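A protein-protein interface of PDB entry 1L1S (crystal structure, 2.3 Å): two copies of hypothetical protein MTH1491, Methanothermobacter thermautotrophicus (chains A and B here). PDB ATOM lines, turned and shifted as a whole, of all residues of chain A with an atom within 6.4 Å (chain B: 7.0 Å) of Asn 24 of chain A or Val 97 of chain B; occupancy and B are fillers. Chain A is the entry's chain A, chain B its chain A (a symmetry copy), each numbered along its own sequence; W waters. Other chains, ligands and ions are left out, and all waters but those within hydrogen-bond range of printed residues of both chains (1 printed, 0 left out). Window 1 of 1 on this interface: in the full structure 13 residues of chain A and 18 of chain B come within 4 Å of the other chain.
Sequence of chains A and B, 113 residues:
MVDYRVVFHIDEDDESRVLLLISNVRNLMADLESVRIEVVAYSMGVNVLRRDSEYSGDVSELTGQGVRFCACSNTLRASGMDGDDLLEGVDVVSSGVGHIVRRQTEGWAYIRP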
ATOM      1  N   PHE A   8      10.284  -0.265 -15.540  1.00  0.00           N
ATOM      2  CA  PHE A   8      10.460   0.427 -14.264  1.00  0.00           C
ATOM      3  C   PHE A   8       9.365   1.445 -14.098  1.00  0.00           C
ATOM      4  O   PHE A   8       8.850   1.985 -15.074  1.00  0.00           O
ATOM      5  CB  PHE A   8      11.797   1.145 -14.178  1.00  0.00           C
ATOM      6  CG  PHE A   8      12.964   0.233 -13.967  1.00  0.00           C
ATOM      7  CD1 PHE A   8      13.505  -0.474 -15.025  1.00  0.00           C
ATOM      8  CD2 PHE A   8      13.534   0.098 -12.701  1.00  0.00           C
ATOM      9  CE1 PHE A   8      14.613  -1.310 -14.832  1.00  0.00           C
ATOM     10  CE2 PHE A   8      14.639  -0.729 -12.489  1.00  0.00           C
ATOM     11  CZ  PHE A   8      15.180  -1.432 -13.556  1.00  0.00           C
ATOM     12  N   LEU A  19      18.149   8.838  -8.754  1.00  0.00           N
ATOM     13  CA  LEU A  19      19.465   8.234  -8.921  1.00  0.00           C
ATOM     14  C   LEU A  19      19.400   6.724  -8.691  1.00  0.00           C
ATOM     15  O   LEU A  19      20.167   5.959  -9.288  1.00  0.00           O
ATOM     16  CB  LEU A  19      20.471   8.892  -7.967  1.00  0.00           C
ATOM     17  CG  LEU A  19      20.779  10.371  -8.292  1.00  0.00           C
ATOM     18  CD1 LEU A  19      21.754  10.968  -7.255  1.00  0.00           C
ATOM     19  CD2 LEU A  19      21.380  10.467  -9.703  1.00  0.00           C
ATOM     20  N   LEU A  20      18.485   6.285  -7.831  1.00  0.00           N
ATOM     21  CA  LEU A  20      18.358   4.852  -7.587  1.00  0.00           C
ATOM     22  C   LEU A  20      17.840   4.158  -8.860  1.00  0.00           C
ATOM     23  O   LEU A  20      18.344   3.105  -9.248  1.00  0.00           O
ATOM     24  CB  LEU A  20      17.422   4.582  -6.404  1.00  0.00           C
ATOM     25  CG  LEU A  20      17.468   3.129  -5.920  1.00  0.00           C
ATOM     26  CD1 LEU A  20      18.918   2.744  -5.660  1.00  0.00           C
ATOM     27  CD2 LEU A  20      16.634   2.960  -4.651  1.00  0.00           C
ATOM     28  N   LEU A  21      16.837   4.748  -9.506  1.00  0.00           N
ATOM     29  CA  LEU A  21      16.296   4.191 -10.747  1.00  0.00           C
ATOM     30  C   LEU A  21      17.405   4.098 -11.796  1.00  0.00           C
ATOM     31  O   LEU A  21      17.605   3.056 -12.424  1.00  0.00           O
ATOM     32  CB  LEU A  21      15.185   5.087 -11.289  1.00  0.00           C
ATOM     33  CG  LEU A  21      14.777   4.929 -12.768  1.00  0.00           C
ATOM     34  CD1 LEU A  21      13.966   3.674 -12.941  1.00  0.00           C
ATOM     35  CD2 LEU A  21      13.945   6.131 -13.217  1.00  0.00           C
ATOM     36  N   ILE A  22      18.103   5.210 -12.001  1.00  0.00           N
ATOM     37  CA  ILE A  22      19.192   5.265 -12.967  1.00  0.00           C
ATOM     38  C   ILE A  22      20.209   4.162 -12.686  1.00  0.00           C
ATOM     39  O   ILE A  22      20.600   3.425 -13.582  1.00  0.00           O
ATOM     40  CB  ILE A  22      19.904   6.623 -12.905  1.00  0.00           C
ATOM     41  CG1 ILE A  22      18.941   7.723 -13.366  1.00  0.00           C
ATOM     42  CG2 ILE A  22      21.171   6.594 -13.773  1.00  0.00           C
ATOM     43  CD1 ILE A  22      19.480   9.109 -13.158  1.00  0.00           C
ATOM     44  N   SER A  23      20.626   4.071 -11.428  1.00  0.00           N
ATOM     45  CA  SER A  23      21.580   3.067 -11.004  1.00  0.00           C
ATOM     46  C   SER A  23      21.039   1.674 -11.265  1.00  0.00           C
ATOM     47  O   SER A  23      21.762   0.808 -11.756  1.00  0.00           O
ATOM     48  CB  SER A  23      21.888   3.221  -9.514  1.00  0.00           C
ATOM     49  OG  SER A  23      22.457   2.021  -9.007  1.00  0.00           O
ATOM     50  N   ASN A  24      19.769   1.454 -10.936  1.00  0.00           N
ATOM     51  CA  ASN A  24      19.156   0.144 -11.162  1.00  0.00           C
ATOM     52  C   ASN A  24      19.123  -0.212 -12.657  1.00  0.00           C
ATOM     53  O   ASN A  24      19.343  -1.364 -13.030  1.00  0.00           O
ATOM     54  CB  ASN A  24      17.739   0.111 -10.588  1.00  0.00           C
ATOM     55  CG  ASN A  24      17.728   0.162  -9.072  1.00  0.00           C
ATOM     56  OD1 ASN A  24      18.727  -0.138  -8.430  1.00  0.00           O
ATOM     57  ND2 ASN A  24      16.595   0.531  -8.495  1.00  0.00           N
ATOM     58  N   VAL A  25      18.845   0.768 -13.512  1.00  0.00           N
ATOM     59  CA  VAL A  25      18.813   0.512 -14.961  1.00  0.00           C
ATOM     60  C   VAL A  25      20.193   0.084 -15.481  1.00  0.00           C
ATOM     61  O   VAL A  25      20.306  -0.870 -16.242  1.00  0.00           O
ATOM     62  CB  VAL A  25      18.356   1.764 -15.744  1.00  0.00           C
ATOM     63  CG1 VAL A  25      18.644   1.600 -17.238  1.00  0.00           C
ATOM     64  CG2 VAL A  25      16.854   1.984 -15.510  1.00  0.00           C
ATOM     65  N   ARG A  26      21.235   0.786 -15.059  1.00  0.00           N
ATOM     66  CA  ARG A  26      22.587   0.448 -15.486  1.00  0.00           C
ATOM     67  C   ARG A  26      23.027  -0.902 -14.924  1.00  0.00           C
ATOM     68  O   ARG A  26      23.605  -1.714 -15.637  1.00  0.00           O
ATOM     69  CB  ARG A  26      23.561   1.541 -15.052  1.00  0.00           C
ATOM     70  CG  ARG A  26      23.427   2.809 -15.865  1.00  0.00           C
ATOM     71  CD  ARG A  26      24.385   3.895 -15.404  1.00  0.00           C
ATOM     72  NE  ARG A  26      24.310   5.049 -16.297  1.00  0.00           N
ATOM     73  CZ  ARG A  26      24.269   6.316 -15.895  1.00  0.00           C
ATOM     74  NH1 ARG A  26      24.302   6.614 -14.603  1.00  0.00           N
ATOM     75  NH2 ARG A  26      24.167   7.287 -16.791  1.00  0.00           N
ATOM     76  N   ASN A  27      22.740  -1.131 -13.647  1.00  0.00           N
ATOM     77  CA  ASN A  27      23.091  -2.380 -12.969  1.00  0.00           C
ATOM     78  C   ASN A  27      22.482  -3.551 -13.735  1.00  0.00           C
ATOM     79  O   ASN A  27      23.146  -4.559 -14.017  1.00  0.00           O
ATOM     80  CB  ASN A  27      22.549  -2.346 -11.532  1.00  0.00           C
ATOM     81  CG  ASN A  27      22.907  -3.594 -10.715  1.00  0.00           C
ATOM     82  OD1 ASN A  27      23.118  -3.512  -9.500  1.00  0.00           O
ATOM     83  ND2 ASN A  27      22.952  -4.746 -11.367  1.00  0.00           N
ATOM     84  N   LEU A  28      21.211  -3.394 -14.076  1.00  0.00           N
ATOM     85  CA  LEU A  28      20.475  -4.408 -14.788  1.00  0.00           C
ATOM     86  C   LEU A  28      21.101  -4.729 -16.145  1.00  0.00           C
ATOM     87  O   LEU A  28      21.242  -5.894 -16.500  1.00  0.00           O
ATOM     88  CB  LEU A  28      19.027  -3.953 -14.949  1.00  0.00           C
ATOM     89  CG  LEU A  28      18.017  -5.005 -15.376  1.00  0.00           C
ATOM     90  CD1 LEU A  28      18.051  -6.182 -14.404  1.00  0.00           C
ATOM     91  CD2 LEU A  28      16.634  -4.383 -15.411  1.00  0.00           C
ATOM     92  N   MET A  29      21.484  -3.706 -16.899  1.00  0.00           N
ATOM     93  CA  MET A  29      22.092  -3.943 -18.208  1.00  0.00           C
ATOM     94  C   MET A  29      23.426  -4.692 -18.136  1.00  0.00           C
ATOM     95  O   MET A  29      23.827  -5.360 -19.089  1.00  0.00           O
ATOM     96  CB  MET A  29      22.291  -2.622 -18.948  1.00  0.00           C
ATOM     97  CG  MET A  29      20.997  -1.946 -19.316  1.00  0.00           C
ATOM     98  SD  MET A  29      21.301  -0.286 -20.286  1.00  0.00           S
ATOM     99  CE  MET A  29      22.271   0.722 -18.954  1.00  0.00           C
ATOM    100  N   ASP A  31      24.204  -6.917 -15.452  1.00  0.00           N
ATOM    101  CA  ASP A  31      24.018  -8.230 -14.823  1.00  0.00           C
ATOM    102  C   ASP A  31      23.244  -9.232 -15.674  1.00  0.00           C
ATOM    103  O   ASP A  31      23.320 -10.439 -15.443  1.00  0.00           O
ATOM    104  CB  ASP A  31      23.318  -8.084 -13.463  1.00  0.00           C
ATOM    105  CG  ASP A  31      23.360  -9.372 -12.641  1.00  0.00           C
ATOM    106  OD1 ASP A  31      24.458  -9.737 -12.159  1.00  0.00           O
ATOM    107  OD2 ASP A  31      22.298 -10.024 -12.484  1.00  0.00           O
ATOM    108  N   LEU A  32      22.496  -8.733 -16.650  1.00  0.00           N
ATOM    109  CA  LEU A  32      21.713  -9.587 -17.539  1.00  0.00           C
ATOM    110  C   LEU A  32      22.277  -9.541 -18.951  1.00  0.00           C
ATOM    111  O   LEU A  32      22.469  -8.463 -19.514  1.00  0.00           O
ATOM    112  CB  LEU A  32      20.254  -9.130 -17.555  1.00  0.00           C
ATOM    113  CG  LEU A  32      19.248  -9.730 -16.565  1.00  0.00           C
ATOM    114  CD1 LEU A  32      19.907 -10.085 -15.239  1.00  0.00           C
ATOM    115  CD2 LEU A  32      18.110  -8.739 -16.376  1.00  0.00           C
ATOM    116  N   ILE A  37      14.528  -2.892 -21.681  1.00  0.00           N
ATOM    117  CA  ILE A  37      14.068  -2.050 -20.586  1.00  0.00           C
ATOM    118  C   ILE A  37      13.240  -0.821 -20.964  1.00  0.00           C
ATOM    119  O   ILE A  37      13.597  -0.082 -21.881  1.00  0.00           O
ATOM    120  CB  ILE A  37      15.250  -1.495 -19.773  1.00  0.00           C
ATOM    121  CG1 ILE A  37      16.205  -2.614 -19.346  1.00  0.00           C
ATOM    122  CG2 ILE A  37      14.720  -0.747 -18.552  1.00  0.00           C
ATOM    123  CD1 ILE A  37      17.394  -2.095 -18.511  1.00  0.00           C
ATOM    124  N   ILE A 111       9.451  -3.459 -11.874  1.00  0.00           N
ATOM    125  CA  ILE A 111      10.317  -2.992 -10.797  1.00  0.00           C
ATOM    126  C   ILE A 111       9.930  -1.574 -10.390  1.00  0.00           C
ATOM    127  O   ILE A 111       9.883  -0.676 -11.220  1.00  0.00           O
ATOM    128  CB  ILE A 111      11.806  -2.980 -11.212  1.00  0.00           C
ATOM    129  CG1 ILE A 111      12.260  -4.385 -11.616  1.00  0.00           C
ATOM    130  CG2 ILE A 111      12.650  -2.471 -10.071  1.00  0.00           C
ATOM    131  CD1 ILE A 111      12.164  -5.396 -10.508  1.00  0.00           C
ATOM    132  N   ARG A 112       9.688  -1.376  -9.100  1.00  0.00           N
ATOM    133  CA  ARG A 112       9.316  -0.069  -8.578  1.00  0.00           C
ATOM    134  C   ARG A 112      10.376   0.354  -7.547  1.00  0.00           C
ATOM    135  O   ARG A 112      10.277   0.048  -6.368  1.00  0.00           O
ATOM    136  CB  ARG A 112       7.913  -0.173  -7.961  1.00  0.00           C
ATOM    137  CG  ARG A 112       7.176   1.156  -7.739  1.00  0.00           C
ATOM    138  CD  ARG A 112       7.685   1.889  -6.519  1.00  0.00           C
ATOM    139  NE  ARG A 112       6.842   3.035  -6.190  1.00  0.00           N
ATOM    140  CZ  ARG A 112       7.211   4.028  -5.386  1.00  0.00           C
ATOM    141  NH1 ARG A 112       8.416   4.015  -4.833  1.00  0.00           N
ATOM    142  NH2 ARG A 112       6.377   5.030  -5.135  1.00  0.00           N
ATOM    143  N   PRO A 113      11.430   1.050  -7.999  1.00  0.00           N
ATOM    144  CA  PRO A 113      12.480   1.477  -7.069  1.00  0.00           C
ATOM    145  C   PRO A 113      11.965   2.448  -6.017  1.00  0.00           C
ATOM    146  O   PRO A 113      12.415   2.379  -4.878  1.00  0.00           O
ATOM    147  CB  PRO A 113      13.522   2.124  -7.981  1.00  0.00           C
ATOM    148  CG  PRO A 113      13.252   1.500  -9.326  1.00  0.00           C
ATOM    149  CD  PRO A 113      11.752   1.477  -9.367  1.00  0.00           C
ATOM    150  N   HIS B   9      11.098  -6.634  -1.965  1.00  0.00           N
ATOM    151  CA  HIS B   9      12.077  -5.662  -2.422  1.00  0.00           C
ATOM    152  C   HIS B   9      12.121  -4.497  -1.457  1.00  0.00           C
ATOM    153  O   HIS B   9      11.103  -3.877  -1.187  1.00  0.00           O
ATOM    154  CB  HIS B   9      11.655  -5.205  -3.826  1.00  0.00           C
ATOM    155  CG  HIS B   9      12.345  -3.978  -4.332  1.00  0.00           C
ATOM    156  ND1 HIS B   9      12.020  -3.406  -5.545  1.00  0.00           N
ATOM    157  CD2 HIS B   9      13.317  -3.198  -3.799  1.00  0.00           C
ATOM    158  CE1 HIS B   9      12.756  -2.327  -5.736  1.00  0.00           C
ATOM    159  NE2 HIS B   9      13.550  -2.177  -4.692  1.00  0.00           N
ATOM    160  N   ASP B  11      14.716  -1.062  -0.574  1.00  0.00           N
ATOM    161  CA  ASP B  11      15.919  -0.307  -0.894  1.00  0.00           C
ATOM    162  C   ASP B  11      16.113   0.924  -0.004  1.00  0.00           C
ATOM    163  O   ASP B  11      16.864   1.837  -0.343  1.00  0.00           O
ATOM    164  CB  ASP B  11      15.931   0.086  -2.385  1.00  0.00           C
ATOM    165  CG  ASP B  11      14.645   0.792  -2.834  1.00  0.00           C
ATOM    166  OD1 ASP B  11      14.331   0.738  -4.048  1.00  0.00           O
ATOM    167  OD2 ASP B  11      13.953   1.403  -1.994  1.00  0.00           O
ATOM    168  N   VAL B  40      15.064  -9.250  -1.027  1.00  0.00           N
ATOM    169  CA  VAL B  40      16.157  -8.616  -1.736  1.00  0.00           C
ATOM    170  C   VAL B  40      16.289  -7.169  -1.289  1.00  0.00           C
ATOM    171  O   VAL B  40      15.378  -6.353  -1.479  1.00  0.00           O
ATOM    172  CB  VAL B  40      15.930  -8.637  -3.263  1.00  0.00           C
ATOM    173  CG1 VAL B  40      17.096  -7.932  -3.973  1.00  0.00           C
ATOM    174  CG2 VAL B  40      15.796 -10.068  -3.749  1.00  0.00           C
ATOM    175  N   TYR B  42      18.774  -3.718  -1.434  1.00  0.00           N
ATOM    176  CA  TYR B  42      19.911  -3.064  -2.066  1.00  0.00           C
ATOM    177  C   TYR B  42      19.916  -1.590  -1.671  1.00  0.00           C
ATOM    178  O   TYR B  42      19.014  -1.138  -0.969  1.00  0.00           O
ATOM    179  CB  TYR B  42      19.924  -3.287  -3.588  1.00  0.00           C
ATOM    180  CG  TYR B  42      18.733  -2.781  -4.378  1.00  0.00           C
ATOM    181  CD1 TYR B  42      18.631  -1.436  -4.743  1.00  0.00           C
ATOM    182  CD2 TYR B  42      17.737  -3.657  -4.808  1.00  0.00           C
ATOM    183  CE1 TYR B  42      17.565  -0.976  -5.529  1.00  0.00           C
ATOM    184  CE2 TYR B  42      16.661  -3.208  -5.593  1.00  0.00           C
ATOM    185  CZ  TYR B  42      16.584  -1.868  -5.948  1.00  0.00           C
ATOM    186  OH  TYR B  42      15.524  -1.415  -6.720  1.00  0.00           O
ATOM    187  N   SER B  43      20.939  -0.858  -2.100  1.00  0.00           N
ATOM    188  CA  SER B  43      21.108   0.543  -1.736  1.00  0.00           C
ATOM    189  C   SER B  43      21.076   0.623  -0.211  1.00  0.00           C
ATOM    190  O   SER B  43      21.590  -0.268   0.474  1.00  0.00           O
ATOM    191  CB  SER B  43      20.006   1.411  -2.341  1.00  0.00           C
ATOM    192  OG  SER B  43      20.176   2.779  -1.978  1.00  0.00           O
ATOM    193  N   CYS B  72      22.926  -7.241  -2.458  1.00  0.00           N
ATOM    194  CA  CYS B  72      23.382  -6.987  -3.816  1.00  0.00           C
ATOM    195  C   CYS B  72      24.902  -6.895  -3.899  1.00  0.00           C
ATOM    196  O   CYS B  72      25.520  -6.033  -3.268  1.00  0.00           O
ATOM    197  CB  CYS B  72      22.746  -5.695  -4.332  1.00  0.00           C
ATOM    198  SG  CYS B  72      23.096  -5.354  -6.048  1.00  0.00           S
ATOM    199  N   ASN B  74      26.788  -5.751  -6.079  1.00  0.00           N
ATOM    200  CA  ASN B  74      27.244  -4.451  -6.573  1.00  0.00           C
ATOM    201  C   ASN B  74      27.127  -3.362  -5.514  1.00  0.00           C
ATOM    202  O   ASN B  74      28.121  -2.728  -5.146  1.00  0.00           O
ATOM    203  CB  ASN B  74      26.434  -4.054  -7.812  1.00  0.00           C
ATOM    204  CG  ASN B  74      26.580  -5.056  -8.950  1.00  0.00           C
ATOM    205  OD1 ASN B  74      25.749  -5.107  -9.862  1.00  0.00           O
ATOM    206  ND2 ASN B  74      27.645  -5.856  -8.904  1.00  0.00           N
ATOM    207  N   THR B  75      25.913  -3.142  -5.021  1.00  0.00           N
ATOM    208  CA  THR B  75      25.707  -2.122  -4.004  1.00  0.00           C
ATOM    209  C   THR B  75      26.749  -2.250  -2.895  1.00  0.00           C
ATOM    210  O   THR B  75      27.319  -1.245  -2.463  1.00  0.00           O
ATOM    211  CB  THR B  75      24.287  -2.209  -3.371  1.00  0.00           C
ATOM    212  OG1 THR B  75      24.165  -3.414  -2.607  1.00  0.00           O
ATOM    213  CG2 THR B  75      23.217  -2.185  -4.459  1.00  0.00           C
ATOM    214  N   VAL B  93      23.710 -12.022  -3.876  1.00  0.00           N
ATOM    215  CA  VAL B  93      23.335 -12.295  -5.254  1.00  0.00           C
ATOM    216  C   VAL B  93      24.161 -11.329  -6.072  1.00  0.00           C
ATOM    217  O   VAL B  93      24.613 -10.309  -5.556  1.00  0.00           O
ATOM    218  CB  VAL B  93      21.818 -12.069  -5.510  1.00  0.00           C
ATOM    219  CG1 VAL B  93      21.016 -13.147  -4.805  1.00  0.00           C
ATOM    220  CG2 VAL B  93      21.395 -10.679  -5.042  1.00  0.00           C
ATOM    221  N   SER B  95      23.252  -9.338  -8.412  1.00  0.00           N
ATOM    222  CA  SER B  95      22.544  -8.071  -8.609  1.00  0.00           C
ATOM    223  C   SER B  95      21.166  -8.112  -7.964  1.00  0.00           C
ATOM    224  O   SER B  95      20.397  -9.040  -8.203  1.00  0.00           O
ATOM    225  CB  SER B  95      22.367  -7.789 -10.095  1.00  0.00           C
ATOM    226  OG  SER B  95      21.386  -6.779 -10.290  1.00  0.00           O
ATOM    227  N   GLY B  96      20.855  -7.102  -7.162  1.00  0.00           N
ATOM    228  CA  GLY B  96      19.561  -7.054  -6.501  1.00  0.00           C
ATOM    229  C   GLY B  96      18.430  -7.009  -7.509  1.00  0.00           C
ATOM    230  O   GLY B  96      17.563  -7.881  -7.503  1.00  0.00           O
ATOM    231  N   VAL B  97      18.438  -6.006  -8.384  1.00  0.00           N
ATOM    232  CA  VAL B  97      17.392  -5.894  -9.393  1.00  0.00           C
ATOM    233  C   VAL B  97      17.401  -7.074 -10.359  1.00  0.00           C
ATOM    234  O   VAL B  97      16.348  -7.566 -10.746  1.00  0.00           O
ATOM    235  CB  VAL B  97      17.497  -4.572 -10.194  1.00  0.00           C
ATOM    236  CG1 VAL B  97      16.954  -3.430  -9.365  1.00  0.00           C
ATOM    237  CG2 VAL B  97      18.943  -4.289 -10.570  1.00  0.00           C
ATOM    238  N   GLY B  98      18.592  -7.530 -10.742  1.00  0.00           N
ATOM    239  CA  GLY B  98      18.684  -8.667 -11.641  1.00  0.00           C
ATOM    240  C   GLY B  98      18.046  -9.902 -11.013  1.00  0.00           C
ATOM    241  O   GLY B  98      17.276 -10.602 -11.658  1.00  0.00           O
ATOM    242  N   HIS B  99      18.359 -10.171  -9.750  1.00  0.00           N
ATOM    243  CA  HIS B  99      17.791 -11.331  -9.074  1.00  0.00           C
ATOM    244  C   HIS B  99      16.262 -11.208  -9.055  1.00  0.00           C
ATOM    245  O   HIS B  99      15.558 -12.181  -9.310  1.00  0.00           O
ATOM    246  CB  HIS B  99      18.322 -11.456  -7.643  1.00  0.00           C
ATOM    247  CG  HIS B  99      17.889 -12.718  -6.958  1.00  0.00           C
ATOM    248  ND1 HIS B  99      18.284 -13.969  -7.386  1.00  0.00           N
ATOM    249  CD2 HIS B  99      17.054 -12.927  -5.910  1.00  0.00           C
ATOM    250  CE1 HIS B  99      17.712 -14.892  -6.634  1.00  0.00           C
ATOM    251  NE2 HIS B  99      16.961 -14.287  -5.731  1.00  0.00           N
ATOM    252  N   ILE B 100      15.759 -10.010  -8.762  1.00  0.00           N
ATOM    253  CA  ILE B 100      14.317  -9.778  -8.737  1.00  0.00           C
ATOM    254  C   ILE B 100      13.703 -10.052 -10.117  1.00  0.00           C
ATOM    255  O   ILE B 100      12.666 -10.709 -10.223  1.00  0.00           O
ATOM    256  CB  ILE B 100      13.989  -8.331  -8.313  1.00  0.00           C
ATOM    257  CG1 ILE B 100      14.392  -8.106  -6.851  1.00  0.00           C
ATOM    258  CG2 ILE B 100      12.494  -8.058  -8.465  1.00  0.00           C
ATOM    259  CD1 ILE B 100      14.182  -6.645  -6.367  1.00  0.00           C
ATOM    260  N   VAL B 101      14.357  -9.581 -11.173  1.00  0.00           N
ATOM    261  CA  VAL B 101      13.841  -9.803 -12.514  1.00  0.00           C
ATOM    262  C   VAL B 101      13.867 -11.284 -12.871  1.00  0.00           C
ATOM    263  O   VAL B 101      12.918 -11.803 -13.463  1.00  0.00           O
ATOM    264  CB  VAL B 101      14.624  -8.981 -13.575  1.00  0.00           C
ATOM    265  CG1 VAL B 101      14.253  -9.445 -14.986  1.00  0.00           C
ATOM    266  CG2 VAL B 101      14.292  -7.492 -13.420  1.00  0.00           C
ATOM    267  N   ARG B 102      14.940 -11.974 -12.503  1.00  0.00           N
ATOM    268  CA  ARG B 102      15.025 -13.406 -12.791  1.00  0.00           C
ATOM    269  C   ARG B 102      13.899 -14.136 -12.057  1.00  0.00           C
ATOM    270  O   ARG B 102      13.221 -14.984 -12.615  1.00  0.00           O
ATOM    271  CB  ARG B 102      16.367 -13.978 -12.324  1.00  0.00           C
ATOM    272  CG  ARG B 102      17.578 -13.458 -13.088  1.00  0.00           C
ATOM    273  CD  ARG B 102      18.788 -14.344 -12.832  1.00  0.00           C
ATOM    274  NE  ARG B 102      19.913 -13.961 -13.681  1.00  0.00           N
ATOM    275  CZ  ARG B 102      20.777 -12.991 -13.395  1.00  0.00           C
ATOM    276  NH1 ARG B 102      20.658 -12.300 -12.272  1.00  0.00           N
ATOM    277  NH2 ARG B 102      21.755 -12.708 -14.242  1.00  0.00           N
ATOM    278  N   ARG B 103      13.722 -13.791 -10.788  1.00  0.00           N
ATOM    279  CA  ARG B 103      12.702 -14.420  -9.973  1.00  0.00           C
ATOM    280  C   ARG B 103      11.307 -14.202 -10.566  1.00  0.00           C
ATOM    281  O   ARG B 103      10.543 -15.147 -10.740  1.00  0.00           O
ATOM    282  CB  ARG B 103      12.780 -13.862  -8.555  1.00  0.00           C
ATOM    283  CG  ARG B 103      12.669 -14.899  -7.478  1.00  0.00           C
ATOM    284  CD  ARG B 103      14.008 -15.480  -6.991  1.00  0.00           C
ATOM    285  NE  ARG B 103      14.459 -16.629  -7.754  1.00  0.00           N
ATOM    286  CZ  ARG B 103      15.291 -17.568  -7.295  1.00  0.00           C
ATOM    287  NH1 ARG B 103      15.774 -17.524  -6.062  1.00  0.00           N
ATOM    288  NH2 ARG B 103      15.670 -18.552  -8.088  1.00  0.00           N
ATOM    289  N   GLN B 104      10.982 -12.950 -10.882  1.00  0.00           N
ATOM    290  CA  GLN B 104       9.684 -12.633 -11.467  1.00  0.00           C
ATOM    291  C   GLN B 104       9.516 -13.417 -12.760  1.00  0.00           C
ATOM    292  O   GLN B 104       8.444 -13.949 -13.051  1.00  0.00           O
ATOM    293  CB  GLN B 104       9.573 -11.134 -11.752  1.00  0.00           C
ATOM    294  CG  GLN B 104       9.144 -10.306 -10.560  1.00  0.00           C
ATOM    295  CD  GLN B 104       8.864  -8.851 -10.912  1.00  0.00           C
ATOM    296  OE1 GLN B 104       8.126  -8.564 -11.841  1.00  0.00           O
ATOM    297  NE2 GLN B 104       9.448  -7.929 -10.150  1.00  0.00           N
HETATM  298  O   HOH W   1      20.546  -3.889  -7.158  1.00  0.00           O
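OH of Tyr 42 of chain B sits at hydrogen-bond distance from ND2 of Asn 24 of chain A, 2.8 Å away.
OD1 of Asp 11 of chain B lies close to O of Pro 113 of chain A (2.7 Å).
OD2 of Asp 31 of chain A is in salt-bridge range of NH1 of Arg 102 of chain B (2.8 Å).
The side-chain amide oxygen (OD1) of Asn 74 of chain B lies close to the side-chain amide oxygen (OD1) of Asn 27 of chain A (3.1 Å).
The side-chain amide nitrogen of Asn 27 of chain A lies within hydrogen-bond range of the side-chain hydroxyl of Ser 95 of chain B (2.8 Å).
SG of Cys 72 of chain B sits close to N of Asn 74 of chain B (3.7 Å).
NE2 of His 9 of chain B is in hydrogen-bond range of OD1 of Asp 11 of chain B (3.1 Å).
A ring nitrogen (NE2) of His 9 of chain B sits at hydrogen-bond distance from the side-chain hydroxyl of Tyr 42 of chain B.
The backbone carbonyl oxygen (O) of Leu 20 of chain A sits close to the side-chain amide nitrogen (ND2) of Asn 24 of chain A, at 3.2 Å.
The backbone carbonyl oxygen of Cys 72 of chain B is in hydrogen-bond range of the side-chain hydroxyl of Thr 75 of chain B (3.0 Å).
Asp 11 of chain B touches Leu 20 of chain A (OD1 to CD2, 3.3 Å).
Tyr 42 of chain B touches Leu 20 of chain A.
Ser 43 of chain B touches Leu 20 of chain A.
Leu 28 of chain A touches Gly 98 of chain B.
Asp 31 of chain A touches Ser 95 of chain B.
Gly 98 of chain B touches Asp 31 of chain A (CA to OD2, 3.95 Å).
CD1 of Ile 111 of chain A touches CG2 of Ile 100 of chain B, at 3.4 Å.
CD1 of Ile 111 of chain A touches NE2 of Gln 104 of chain B, at 3.7 Å.
Arg 112 of chain A touches His 9 of chain B.
Phe 8 of chain A touches none of the printed residues of chain B.
Of chain B, only Tyr 42 (2.8 Å) and Val 97 (3.7 Å) come within 4 Å of Asn 24 of chain A.
Of the printed residues of chain B, Asn 27 of chain A touches Cys 72 (3.9 Å), Asn 74 (3.1 Å) and Ser 95 (2.8 Å).
Of the printed residues of chain A, Asp 11 of chain B touches Leu 20 and Pro 113.
Of the printed residues of chain A, Ser 43 of chain B touches Leu 20.
Printed residues of chain A within 4 Å of Asn 74 of chain B: Asn 27.
Printed residues of chain A within 4 Å of Val 97 of chain B: Asn 24 (3.7 Å).
The nearest residue of chain B that does not touch Asn 24 of chain A is Asp 11 of chain B (5.0 Å).
The nearest residue of chain A that does not touch Val 97 of chain B is Asn 27 of chain A (4.03 Å).
The nearest printed residue of chain A that does not touch Ser 43 of chain B is Asn 24 of chain A (6.4 Å).
Of the 19 printed residues of chain B, 12 touch a printed residue of chain A.
Printed residues of chain B that touch a printed residue of chain A: His 9, Asp 11, Tyr 42, Ser 43, Cys 72, Asn 74, Ser 95, Val 97, Gly 98, Ile 100, Arg 102 and Gln 104.
Of the 18 printed residues of chain A, 9 touch a printed residue of chain B.
Hydrophobic or aromatic side chains of chain A that line the printed part of chain B: Leu 20, Leu 28, Leu 32 and Ile 111.
Along chain A the printed residues that touch a printed residue of chain B span positions 20 to 113.
Among the printed residues, 17 pairs touch across the chains.
No position is printed for both chains.
Of the 17 pairs that touch across the chains among the printed residues, none has its exchanged pair printed and touching as well.
Water W1 lies within hydrogen-bond range of the side-chain sulfur of Cys 72 of chain B (3.1 Å), the backbone NH of Gly 96 of chain B (3.2 Å), the backbone NH of Val 97 of chain B (3.2 Å) and the side-chain amide oxygen of Asn 27 of chain A (3.5 Å).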
